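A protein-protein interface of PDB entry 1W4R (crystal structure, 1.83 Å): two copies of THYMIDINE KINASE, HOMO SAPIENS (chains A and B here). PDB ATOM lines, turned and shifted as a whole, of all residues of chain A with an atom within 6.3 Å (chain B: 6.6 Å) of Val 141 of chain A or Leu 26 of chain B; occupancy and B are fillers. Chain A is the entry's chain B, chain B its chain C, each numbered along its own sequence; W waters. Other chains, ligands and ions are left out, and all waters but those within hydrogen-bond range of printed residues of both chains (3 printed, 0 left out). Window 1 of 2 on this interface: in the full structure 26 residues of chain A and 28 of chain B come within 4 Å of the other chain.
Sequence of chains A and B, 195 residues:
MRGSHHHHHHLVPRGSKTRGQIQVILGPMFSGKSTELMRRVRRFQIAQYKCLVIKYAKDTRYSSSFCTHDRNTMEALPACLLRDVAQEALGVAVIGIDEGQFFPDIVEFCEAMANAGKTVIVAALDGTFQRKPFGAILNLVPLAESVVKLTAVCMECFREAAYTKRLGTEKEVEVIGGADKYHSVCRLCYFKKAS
Printed residues of chain B within 4 Å of Leu 26 of chain A: Val 141 (3.9 Å).
Val 141 of chain A touches just these residues of chain B: Leu 26, Asp 126, Leu 138 and Lys 149.
Leu 26 of chain B touches one residue of chain A.
Of the printed residues of chain A, Asp 126 of chain B touches Val 141 (3.1 Å) and Pro 142 (3.2 Å).
Thr 151 of chain B touches none of the printed residues of chain A.
The nearest residue of chain B that does not touch Val 141 of chain A is Val 141 of chain B (5.5 Å).
Water W1 bridges O of Lys 149 of chain B (2.8 Å) and N of Val 147 of chain A (3.0 Å).
Water W3 bridges O of Val 147 of chain A (2.8 Å) and N of Lys 149 of chain B (3.1 Å).
Water W2 bridges the backbone carbonyl oxygen (O) of Leu 150 of chain B (3.0 Å) and the backbone carbonyl oxygen (O) of Glu 145 of chain A (3.2 Å).
The backbone carbonyl oxygen (O) of Val 141 of chain A sits at hydrogen-bond distance from the side-chain amino group (NZ) of Lys 149 of chain B (3.1 Å).
O of Leu 143 of chain A sits at hydrogen-bond distance from OH of Tyr 163 of chain B.
The backbone carbonyl oxygen of Ala 144 of chain A is in hydrogen-bond range of the side-chain amino group of Lys 149 of chain B (2.8 Å).
OH of Tyr 163 of chain B is in hydrogen-bond range of OE1 of Glu 145 of chain A, at 2.9 Å.
O of Val 141 of chain A sits close to OD2 of Asp 126 of chain B (3.1 Å).
Printed residues of chain A that touch a printed residue of chain B: Leu 26, Leu 138, Val 141, Pro 142, Leu 143, Ala 144, Glu 145 and Val 147.
Hydrophobic or aromatic side chains of chain A within 4 Å of the printed part of chain B: Leu 26, Leu 138, Val 141, Pro 142 and Val 147.
Of the 23 printed residues of chain B, 8 touch a printed residue of chain A.
Among the printed residues, 18 pairs touch across the chains.
Leu 26 of chain A touches Val 141 of chain B, and with the chains exchanged Val 141 of chain A touches Leu 26 of chain B.
Leu 138 of chain B touches its own counterpart, Leu 138 of chain A.
Leu 138 of chain A touches Val 141 of chain B, and with the chains exchanged Val 141 of chain A touches Leu 138 of chain B.
6 positions are printed for both chains.
CD1 of Leu 138 of chain B touches O of Leu 138 of chain A (3.2 Å).
CD2 of Leu 138 of chain A touches CG1 of Val 141 of chain B, 3.8 Å away.
CG1 of Val 141 of chain A touches CD1 of Leu 26 of chain B (3.8 Å).
Leu 138 of chain B touches Val 141 of chain A (CD2 to CG1, 3.9 Å).
OD2 of Asp 126 of chain B touches CA of Pro 142 of chain A, 3.2 Å away.
Leu 138 of chain B touches Pro 142 of chain A.
Ala 144 of chain A touches Ala 162 of chain B.
C of Ala 144 of chain A touches OH of Tyr 163 of chain B, at 3.6 Å.
Ala 162 of chain B touches Glu 145 of chain A (CB to CA, 3.7 Å).
N of Lys 149 of chain B touches O of Val 147 of chain A (3.6 Å).
The backbone NH (N) of Leu 26 of chain B sits at hydrogen-bond distance from the backbone carbonyl oxygen (O) of Val 148 of chain B, 2.8 Å away.
The backbone carbonyl oxygen (O) of Leu 26 of chain B lies within hydrogen-bond range of the backbone NH (N) of Leu 150 of chain B, 2.8 Å away.
NZ of Lys 149 of chain B lies within salt-bridge range of OD2 of Asp 126 of chain B (2.7 Å).
The side-chain amino group (NZ) of Lys 149 of chain B is in hydrogen-bond range of the backbone carbonyl oxygen (O) of Ala 162 of chain B.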
ATOM      1  N   VAL A  24     -19.724  10.723  -4.311  1.00  0.00           N
ATOM      2  CA  VAL A  24     -19.088  10.201  -3.133  1.00  0.00           C
ATOM      3  C   VAL A  24     -19.428   8.718  -2.966  1.00  0.00           C
ATOM      4  O   VAL A  24     -20.600   8.316  -3.007  1.00  0.00           O
ATOM      5  CB  VAL A  24     -19.534  10.940  -1.868  1.00  0.00           C
ATOM      6  CG1 VAL A  24     -18.708  10.471  -0.670  1.00  0.00           C
ATOM      7  CG2 VAL A  24     -19.344  12.463  -2.028  1.00  0.00           C
ATOM      8  N   LEU A  26     -18.848   5.943  -0.296  1.00  0.00           N
ATOM      9  CA  LEU A  26     -18.524   5.651   1.079  1.00  0.00           C
ATOM     10  C   LEU A  26     -18.545   4.166   1.321  1.00  0.00           C
ATOM     11  O   LEU A  26     -18.995   3.399   0.504  1.00  0.00           O
ATOM     12  CB  LEU A  26     -19.496   6.332   2.030  1.00  0.00           C
ATOM     13  CG  LEU A  26     -19.545   7.858   1.889  1.00  0.00           C
ATOM     14  CD1 LEU A  26     -20.729   8.396   2.672  1.00  0.00           C
ATOM     15  CD2 LEU A  26     -18.242   8.500   2.342  1.00  0.00           C
ATOM     16  N   ILE A 137     -15.007  14.398   5.852  1.00  0.00           N
ATOM     17  CA  ILE A 137     -15.584  13.762   4.681  1.00  0.00           C
ATOM     18  C   ILE A 137     -17.078  13.939   4.549  1.00  0.00           C
ATOM     19  O   ILE A 137     -17.571  14.141   3.447  1.00  0.00           O
ATOM     20  CB  ILE A 137     -15.229  12.252   4.626  1.00  0.00           C
ATOM     21  CG1 ILE A 137     -15.539  11.736   3.235  1.00  0.00           C
ATOM     22  CG2 ILE A 137     -15.994  11.472   5.670  1.00  0.00           C
ATOM     23  CD1 ILE A 137     -14.674  12.359   2.199  1.00  0.00           C
ATOM     24  N   LEU A 138     -17.813  13.882   5.644  1.00  0.00           N
ATOM     25  CA  LEU A 138     -19.251  13.895   5.533  1.00  0.00           C
ATOM     26  C   LEU A 138     -19.799  15.265   5.172  1.00  0.00           C
ATOM     27  O   LEU A 138     -20.934  15.370   4.746  1.00  0.00           O
ATOM     28  CB  LEU A 138     -19.897  13.386   6.788  1.00  0.00           C
ATOM     29  CG  LEU A 138     -19.554  11.918   7.086  1.00  0.00           C
ATOM     30  CD1 LEU A 138     -20.210  11.581   8.360  1.00  0.00           C
ATOM     31  CD2 LEU A 138     -19.972  10.937   6.019  1.00  0.00           C
ATOM     32  N   ASN A 139     -18.983  16.300   5.289  1.00  0.00           N
ATOM     33  CA  ASN A 139     -19.396  17.610   4.808  1.00  0.00           C
ATOM     34  C   ASN A 139     -19.505  17.653   3.291  1.00  0.00           C
ATOM     35  O   ASN A 139     -20.115  18.582   2.781  1.00  0.00           O
ATOM     36  CB  ASN A 139     -18.455  18.717   5.304  1.00  0.00           C
ATOM     37  CG  ASN A 139     -18.511  18.889   6.815  1.00  0.00           C
ATOM     38  OD1 ASN A 139     -19.571  19.023   7.391  1.00  0.00           O
ATOM     39  ND2 ASN A 139     -17.372  18.844   7.450  1.00  0.00           N
ATOM     40  N   LEU A 140     -18.970  16.648   2.569  1.00  0.00           N
ATOM     41  CA  LEU A 140     -19.204  16.533   1.123  1.00  0.00           C
ATOM     42  C   LEU A 140     -20.613  16.161   0.790  1.00  0.00           C
ATOM     43  O   LEU A 140     -21.062  16.440  -0.298  1.00  0.00           O
ATOM     44  CB  LEU A 140     -18.323  15.466   0.434  1.00  0.00           C
ATOM     45  CG  LEU A 140     -16.874  15.751   0.190  1.00  0.00           C
ATOM     46  CD1 LEU A 140     -16.289  14.557  -0.577  1.00  0.00           C
ATOM     47  CD2 LEU A 140     -16.660  17.011  -0.566  1.00  0.00           C
ATOM     48  N   VAL A 141     -21.294  15.458   1.690  1.00  0.00           N
ATOM     49  CA  VAL A 141     -22.562  14.855   1.367  1.00  0.00           C
ATOM     50  C   VAL A 141     -23.592  15.891   0.869  1.00  0.00           C
ATOM     51  O   VAL A 141     -24.199  15.705  -0.179  1.00  0.00           O
ATOM     52  CB  VAL A 141     -23.097  13.993   2.532  1.00  0.00           C
ATOM     53  CG1 VAL A 141     -24.504  13.548   2.267  1.00  0.00           C
ATOM     54  CG2 VAL A 141     -22.163  12.800   2.793  1.00  0.00           C
ATOM     55  N   PRO A 142     -23.793  16.977   1.607  1.00  0.00           N
ATOM     56  CA  PRO A 142     -24.710  18.022   1.150  1.00  0.00           C
ATOM     57  C   PRO A 142     -24.254  18.729  -0.103  1.00  0.00           C
ATOM     58  O   PRO A 142     -25.105  19.357  -0.742  1.00  0.00           O
ATOM     59  CB  PRO A 142     -24.739  19.032   2.310  1.00  0.00           C
ATOM     60  CG  PRO A 142     -24.186  18.292   3.482  1.00  0.00           C
ATOM     61  CD  PRO A 142     -23.220  17.280   2.924  1.00  0.00           C
ATOM     62  N   LEU A 143     -22.973  18.693  -0.426  1.00  0.00           N
ATOM     63  CA  LEU A 143     -22.470  19.256  -1.671  1.00  0.00           C
ATOM     64  C   LEU A 143     -22.529  18.315  -2.874  1.00  0.00           C
ATOM     65  O   LEU A 143     -22.312  18.737  -3.998  1.00  0.00           O
ATOM     66  CB  LEU A 143     -21.026  19.687  -1.479  1.00  0.00           C
ATOM     67  CG  LEU A 143     -20.803  20.567  -0.257  1.00  0.00           C
ATOM     68  CD1 LEU A 143     -19.322  20.711  -0.003  1.00  0.00           C
ATOM     69  CD2 LEU A 143     -21.468  21.917  -0.477  1.00  0.00           C
ATOM     70  N   ALA A 144     -22.821  17.048  -2.641  1.00  0.00           N
ATOM     71  CA  ALA A 144     -22.678  16.022  -3.672  1.00  0.00           C
ATOM     72  C   ALA A 144     -23.948  15.661  -4.423  1.00  0.00           C
ATOM     73  O   ALA A 144     -25.016  15.540  -3.858  1.00  0.00           O
ATOM     74  CB  ALA A 144     -22.111  14.786  -3.067  1.00  0.00           C
ATOM     75  N   GLU A 145     -23.783  15.433  -5.712  1.00  0.00           N
ATOM     76  CA  GLU A 145     -24.833  14.981  -6.593  1.00  0.00           C
ATOM     77  C   GLU A 145     -25.200  13.521  -6.386  1.00  0.00           C
ATOM     78  O   GLU A 145     -26.318  13.120  -6.669  1.00  0.00           O
ATOM     79  CB  GLU A 145     -24.345  15.188  -8.057  1.00  0.00           C
ATOM     80  CG  GLU A 145     -24.583  16.627  -8.537  1.00  0.00           C
ATOM     81  CD  GLU A 145     -23.467  17.625  -8.285  1.00  0.00           C
ATOM     82  OE1 GLU A 145     -22.499  17.389  -7.499  1.00  0.00           O
ATOM     83  OE2 GLU A 145     -23.572  18.732  -8.885  1.00  0.00           O
ATOM     84  N   VAL A 147     -24.305  10.025  -3.747  1.00  0.00           N
ATOM     85  CA  VAL A 147     -23.663   9.439  -2.558  1.00  0.00           C
ATOM     86  C   VAL A 147     -24.141   8.012  -2.441  1.00  0.00           C
ATOM     87  O   VAL A 147     -25.331   7.766  -2.458  1.00  0.00           O
ATOM     88  CB  VAL A 147     -24.037  10.243  -1.272  1.00  0.00           C
ATOM     89  CG1 VAL A 147     -23.388   9.632  -0.029  1.00  0.00           C
ATOM     90  CG2 VAL A 147     -23.607  11.716  -1.432  1.00  0.00           C
ATOM     91  N   VAL B  24     -30.563   4.941   6.035  1.00  0.00           N
ATOM     92  CA  VAL B  24     -30.744   6.352   5.914  1.00  0.00           C
ATOM     93  C   VAL B  24     -31.060   6.676   4.454  1.00  0.00           C
ATOM     94  O   VAL B  24     -30.356   6.217   3.552  1.00  0.00           O
ATOM     95  CB  VAL B  24     -29.484   7.111   6.311  1.00  0.00           C
ATOM     96  CG1 VAL B  24     -29.719   8.594   6.244  1.00  0.00           C
ATOM     97  CG2 VAL B  24     -29.015   6.710   7.712  1.00  0.00           C
ATOM     98  N   ILE B  25     -32.099   7.469   4.253  1.00  0.00           N
ATOM     99  CA  ILE B  25     -32.591   7.893   2.933  1.00  0.00           C
ATOM    100  C   ILE B  25     -32.419   9.378   2.917  1.00  0.00           C
ATOM    101  O   ILE B  25     -33.206  10.138   3.542  1.00  0.00           O
ATOM    102  CB  ILE B  25     -34.060   7.548   2.758  1.00  0.00           C
ATOM    103  CG1 ILE B  25     -34.301   6.057   2.895  1.00  0.00           C
ATOM    104  CG2 ILE B  25     -34.555   8.013   1.377  1.00  0.00           C
ATOM    105  CD1 ILE B  25     -35.718   5.710   3.090  1.00  0.00           C
ATOM    106  N   LEU B  26     -31.359   9.817   2.264  1.00  0.00           N
ATOM    107  CA  LEU B  26     -31.063  11.225   2.120  1.00  0.00           C
ATOM    108  C   LEU B  26     -31.548  11.779   0.814  1.00  0.00           C
ATOM    109  O   LEU B  26     -31.909  11.036  -0.099  1.00  0.00           O
ATOM    110  CB  LEU B  26     -29.572  11.420   2.195  1.00  0.00           C
ATOM    111  CG  LEU B  26     -28.882  11.009   3.490  1.00  0.00           C
ATOM    112  CD1 LEU B  26     -27.383  11.238   3.344  1.00  0.00           C
ATOM    113  CD2 LEU B  26     -29.460  11.764   4.690  1.00  0.00           C
ATOM    114  N   GLY B  27     -31.546  13.094   0.683  1.00  0.00           N
ATOM    115  CA  GLY B  27     -31.844  13.712  -0.596  1.00  0.00           C
ATOM    116  C   GLY B  27     -32.330  15.132  -0.397  1.00  0.00           C
ATOM    117  O   GLY B  27     -32.566  15.524   0.757  1.00  0.00           O
ATOM    118  N   PRO B  28     -32.485  15.883  -1.475  1.00  0.00           N
ATOM    119  CA  PRO B  28     -33.049  17.235  -1.374  1.00  0.00           C
ATOM    120  C   PRO B  28     -34.558  17.136  -1.178  1.00  0.00           C
ATOM    121  O   PRO B  28     -35.125  16.039  -1.073  1.00  0.00           O
ATOM    122  CB  PRO B  28     -32.691  17.856  -2.716  1.00  0.00           C
ATOM    123  CG  PRO B  28     -32.776  16.701  -3.642  1.00  0.00           C
ATOM    124  CD  PRO B  28     -32.259  15.506  -2.885  1.00  0.00           C
ATOM    125  N   SER B  31     -37.687  14.881  -3.556  1.00  0.00           N
ATOM    126  CA  SER B  31     -37.048  13.671  -4.116  1.00  0.00           C
ATOM    127  C   SER B  31     -37.783  12.412  -3.697  1.00  0.00           C
ATOM    128  O   SER B  31     -37.419  11.282  -4.081  1.00  0.00           O
ATOM    129  CB  SER B  31     -35.590  13.633  -3.698  1.00  0.00           C
ATOM    130  OG  SER B  31     -35.453  13.607  -2.289  1.00  0.00           O
ATOM    131  N   LYS B  33     -38.337  11.205  -0.510  1.00  0.00           N
ATOM    132  CA  LYS B  33     -37.737  10.491   0.625  1.00  0.00           C
ATOM    133  C   LYS B  33     -38.770   9.825   1.482  1.00  0.00           C
ATOM    134  O   LYS B  33     -38.600   8.686   1.883  1.00  0.00           O
ATOM    135  CB  LYS B  33     -36.908  11.427   1.505  1.00  0.00           C
ATOM    136  CG  LYS B  33     -35.805  12.163   0.731  1.00  0.00           C
ATOM    137  CD  LYS B  33     -34.977  13.123   1.581  1.00  0.00           C
ATOM    138  CE  LYS B  33     -35.783  14.250   2.187  1.00  0.00           C
ATOM    139  NZ  LYS B  33     -36.435  15.147   1.180  1.00  0.00           N
ATOM    140  N   VAL B 122     -34.610   5.992   8.312  1.00  0.00           N
ATOM    141  CA  VAL B 122     -34.702   7.427   8.505  1.00  0.00           C
ATOM    142  C   VAL B 122     -34.685   8.129   7.175  1.00  0.00           C
ATOM    143  O   VAL B 122     -33.751   7.950   6.395  1.00  0.00           O
ATOM    144  CB  VAL B 122     -33.519   7.985   9.340  1.00  0.00           C
ATOM    145  CG1 VAL B 122     -33.646   9.483   9.556  1.00  0.00           C
ATOM    146  CG2 VAL B 122     -33.389   7.243  10.672  1.00  0.00           C
ATOM    147  N   ALA B 123     -35.705   8.936   6.926  1.00  0.00           N
ATOM    148  CA  ALA B 123     -35.688   9.866   5.805  1.00  0.00           C
ATOM    149  C   ALA B 123     -35.304  11.241   6.296  1.00  0.00           C
ATOM    150  O   ALA B 123     -35.795  11.697   7.343  1.00  0.00           O
ATOM    151  CB  ALA B 123     -37.036   9.862   5.158  1.00  0.00           C
ATOM    152  N   ALA B 124     -34.404  11.914   5.581  1.00  0.00           N
ATOM    153  CA  ALA B 124     -33.954  13.242   5.977  1.00  0.00           C
ATOM    154  C   ALA B 124     -33.295  13.986   4.869  1.00  0.00           C
ATOM    155  O   ALA B 124     -32.643  13.380   4.011  1.00  0.00           O
ATOM    156  CB  ALA B 124     -32.972  13.143   7.160  1.00  0.00           C
ATOM    157  N   LEU B 125     -33.405  15.308   4.920  1.00  0.00           N
ATOM    158  CA  LEU B 125     -32.567  16.150   4.112  1.00  0.00           C
ATOM    159  C   LEU B 125     -31.151  16.048   4.584  1.00  0.00           C
ATOM    160  O   LEU B 125     -30.888  16.048   5.778  1.00  0.00           O
ATOM    161  CB  LEU B 125     -32.980  17.597   4.199  1.00  0.00           C
ATOM    162  CG  LEU B 125     -34.364  17.921   3.649  1.00  0.00           C
ATOM    163  CD1 LEU B 125     -34.708  19.326   4.105  1.00  0.00           C
ATOM    164  CD2 LEU B 125     -34.399  17.857   2.153  1.00  0.00           C
ATOM    165  N   ASP B 126     -30.235  15.918   3.634  1.00  0.00           N
ATOM    166  CA  ASP B 126     -28.821  15.927   3.959  1.00  0.00           C
ATOM    167  C   ASP B 126     -28.279  17.336   4.111  1.00  0.00           C
ATOM    168  O   ASP B 126     -27.376  17.587   4.928  1.00  0.00           O
ATOM    169  CB  ASP B 126     -28.034  15.138   2.925  1.00  0.00           C
ATOM    170  CG  ASP B 126     -28.149  15.698   1.561  1.00  0.00           C
ATOM    171  OD1 ASP B 126     -29.289  15.951   1.081  1.00  0.00           O
ATOM    172  OD2 ASP B 126     -27.134  15.907   0.879  1.00  0.00           O
ATOM    173  N   GLY B 127     -28.845  18.269   3.351  1.00  0.00           N
ATOM    174  CA  GLY B 127     -28.427  19.632   3.409  1.00  0.00           C
ATOM    175  C   GLY B 127     -29.542  20.625   3.610  1.00  0.00           C
ATOM    176  O   GLY B 127     -30.684  20.405   3.204  1.00  0.00           O
ATOM    177  N   ILE B 137     -27.935  14.939  11.329  1.00  0.00           N
ATOM    178  CA  ILE B 137     -28.311  13.783  10.551  1.00  0.00           C
ATOM    179  C   ILE B 137     -27.096  13.049   9.951  1.00  0.00           C
ATOM    180  O   ILE B 137     -27.104  11.836   9.887  1.00  0.00           O
ATOM    181  CB  ILE B 137     -29.339  14.203   9.475  1.00  0.00           C
ATOM    182  CG1 ILE B 137     -30.047  12.988   8.938  1.00  0.00           C
ATOM    183  CG2 ILE B 137     -28.661  14.964   8.399  1.00  0.00           C
ATOM    184  CD1 ILE B 137     -30.972  12.388   9.940  1.00  0.00           C
ATOM    185  N   LEU B 138     -26.061  13.760   9.539  1.00  0.00           N
ATOM    186  CA  LEU B 138     -24.918  13.106   8.892  1.00  0.00           C
ATOM    187  C   LEU B 138     -24.105  12.258   9.869  1.00  0.00           C
ATOM    188  O   LEU B 138     -23.475  11.294   9.460  1.00  0.00           O
ATOM    189  CB  LEU B 138     -24.043  14.091   8.132  1.00  0.00           C
ATOM    190  CG  LEU B 138     -24.763  14.768   6.948  1.00  0.00           C
ATOM    191  CD1 LEU B 138     -23.834  15.652   6.142  1.00  0.00           C
ATOM    192  CD2 LEU B 138     -25.441  13.770   6.035  1.00  0.00           C
ATOM    193  N   VAL B 141     -24.456   8.535   9.437  1.00  0.00           N
ATOM    194  CA  VAL B 141     -23.886   7.813   8.297  1.00  0.00           C
ATOM    195  C   VAL B 141     -22.844   6.768   8.763  1.00  0.00           C
ATOM    196  O   VAL B 141     -22.922   5.614   8.380  1.00  0.00           O
ATOM    197  CB  VAL B 141     -23.314   8.800   7.260  1.00  0.00           C
ATOM    198  CG1 VAL B 141     -22.468   8.103   6.190  1.00  0.00           C
ATOM    199  CG2 VAL B 141     -24.465   9.516   6.592  1.00  0.00           C
ATOM    200  N   VAL B 147     -27.005   3.632   3.293  1.00  0.00           N
ATOM    201  CA  VAL B 147     -27.187   5.041   3.047  1.00  0.00           C
ATOM    202  C   VAL B 147     -27.361   5.252   1.545  1.00  0.00           C
ATOM    203  O   VAL B 147     -26.532   4.801   0.761  1.00  0.00           O
ATOM    204  CB  VAL B 147     -25.984   5.891   3.507  1.00  0.00           C
ATOM    205  CG1 VAL B 147     -26.264   7.400   3.323  1.00  0.00           C
ATOM    206  CG2 VAL B 147     -25.633   5.584   4.976  1.00  0.00           C
ATOM    207  N   VAL B 148     -28.421   5.953   1.163  1.00  0.00           N
ATOM    208  CA  VAL B 148     -28.643   6.360  -0.230  1.00  0.00           C
ATOM    209  C   VAL B 148     -29.013   7.840  -0.270  1.00  0.00           C
ATOM    210  O   VAL B 148     -29.507   8.372   0.717  1.00  0.00           O
ATOM    211  CB  VAL B 148     -29.803   5.551  -0.916  1.00  0.00           C
ATOM    212  CG1 VAL B 148     -29.561   4.048  -0.944  1.00  0.00           C
ATOM    213  CG2 VAL B 148     -31.125   5.819  -0.263  1.00  0.00           C
ATOM    214  N   LYS B 149     -28.681   8.529  -1.357  1.00  0.00           N
ATOM    215  CA  LYS B 149     -29.088   9.908  -1.561  1.00  0.00           C
ATOM    216  C   LYS B 149     -29.949   9.918  -2.837  1.00  0.00           C
ATOM    217  O   LYS B 149     -29.504   9.501  -3.898  1.00  0.00           O
ATOM    218  CB  LYS B 149     -27.925  10.866  -1.725  1.00  0.00           C
ATOM    219  CG  LYS B 149     -28.365  12.328  -1.825  1.00  0.00           C
ATOM    220  CD  LYS B 149     -27.265  13.351  -1.763  1.00  0.00           C
ATOM    221  CE  LYS B 149     -27.816  14.749  -2.009  1.00  0.00           C
ATOM    222  NZ  LYS B 149     -26.869  15.913  -1.795  1.00  0.00           N
ATOM    223  N   LEU B 150     -31.205  10.283  -2.689  1.00  0.00           N
ATOM    224  CA  LEU B 150     -32.131  10.340  -3.815  1.00  0.00           C
ATOM    225  C   LEU B 150     -31.942  11.655  -4.538  1.00  0.00           C
ATOM    226  O   LEU B 150     -31.315  12.603  -3.999  1.00  0.00           O
ATOM    227  CB  LEU B 150     -33.562  10.198  -3.314  1.00  0.00           C
ATOM    228  CG  LEU B 150     -33.891   8.992  -2.451  1.00  0.00           C
ATOM    229  CD1 LEU B 150     -35.323   9.064  -2.054  1.00  0.00           C
ATOM    230  CD2 LEU B 150     -33.608   7.718  -3.181  1.00  0.00           C
ATOM    231  N   THR B 151     -32.472  11.727  -5.757  1.00  0.00           N
ATOM    232  CA  THR B 151     -32.478  12.958  -6.538  1.00  0.00           C
ATOM    233  C   THR B 151     -33.912  13.421  -6.799  1.00  0.00           C
ATOM    234  O   THR B 151     -34.872  12.637  -6.827  1.00  0.00           O
ATOM    235  CB  THR B 151     -31.817  12.758  -7.929  1.00  0.00           C
ATOM    236  OG1 THR B 151     -32.575  11.773  -8.646  1.00  0.00           O
ATOM    237  CG2 THR B 151     -30.403  12.198  -7.817  1.00  0.00           C
ATOM    238  N   ALA B 162     -29.851  17.798  -6.851  1.00  0.00           N
ATOM    239  CA  ALA B 162     -29.351  17.254  -5.597  1.00  0.00           C
ATOM    240  C   ALA B 162     -29.489  18.190  -4.414  1.00  0.00           C
ATOM    241  O   ALA B 162     -29.173  17.798  -3.262  1.00  0.00           O
ATOM    242  CB  ALA B 162     -27.919  16.861  -5.788  1.00  0.00           C
ATOM    243  N   TYR B 163     -29.937  19.426  -4.664  1.00  0.00           N
ATOM    244  CA  TYR B 163     -29.953  20.450  -3.639  1.00  0.00           C
ATOM    245  C   TYR B 163     -31.332  21.113  -3.542  1.00  0.00           C
ATOM    246  O   TYR B 163     -32.202  20.911  -4.404  1.00  0.00           O
ATOM    247  CB  TYR B 163     -28.897  21.514  -3.943  1.00  0.00           C
ATOM    248  CG  TYR B 163     -27.618  20.891  -4.436  1.00  0.00           C
ATOM    249  CD1 TYR B 163     -26.834  20.133  -3.586  1.00  0.00           C
ATOM    250  CD2 TYR B 163     -27.266  20.975  -5.785  1.00  0.00           C
ATOM    251  CE1 TYR B 163     -25.700  19.534  -4.032  1.00  0.00           C
ATOM    252  CE2 TYR B 163     -26.140  20.369  -6.256  1.00  0.00           C
ATOM    253  CZ  TYR B 163     -25.342  19.656  -5.366  1.00  0.00           C
ATOM    254  OH  TYR B 163     -24.231  19.011  -5.812  1.00  0.00           O
HETATM  255  O   HOH W   1     -26.955   9.284  -4.953  1.00  0.00           O
HETATM  256  O   HOH W   2     -29.055  14.024  -5.278  1.00  0.00           O
HETATM  257  O   HOH W   3     -27.623   6.467  -3.367  1.00  0.00           O
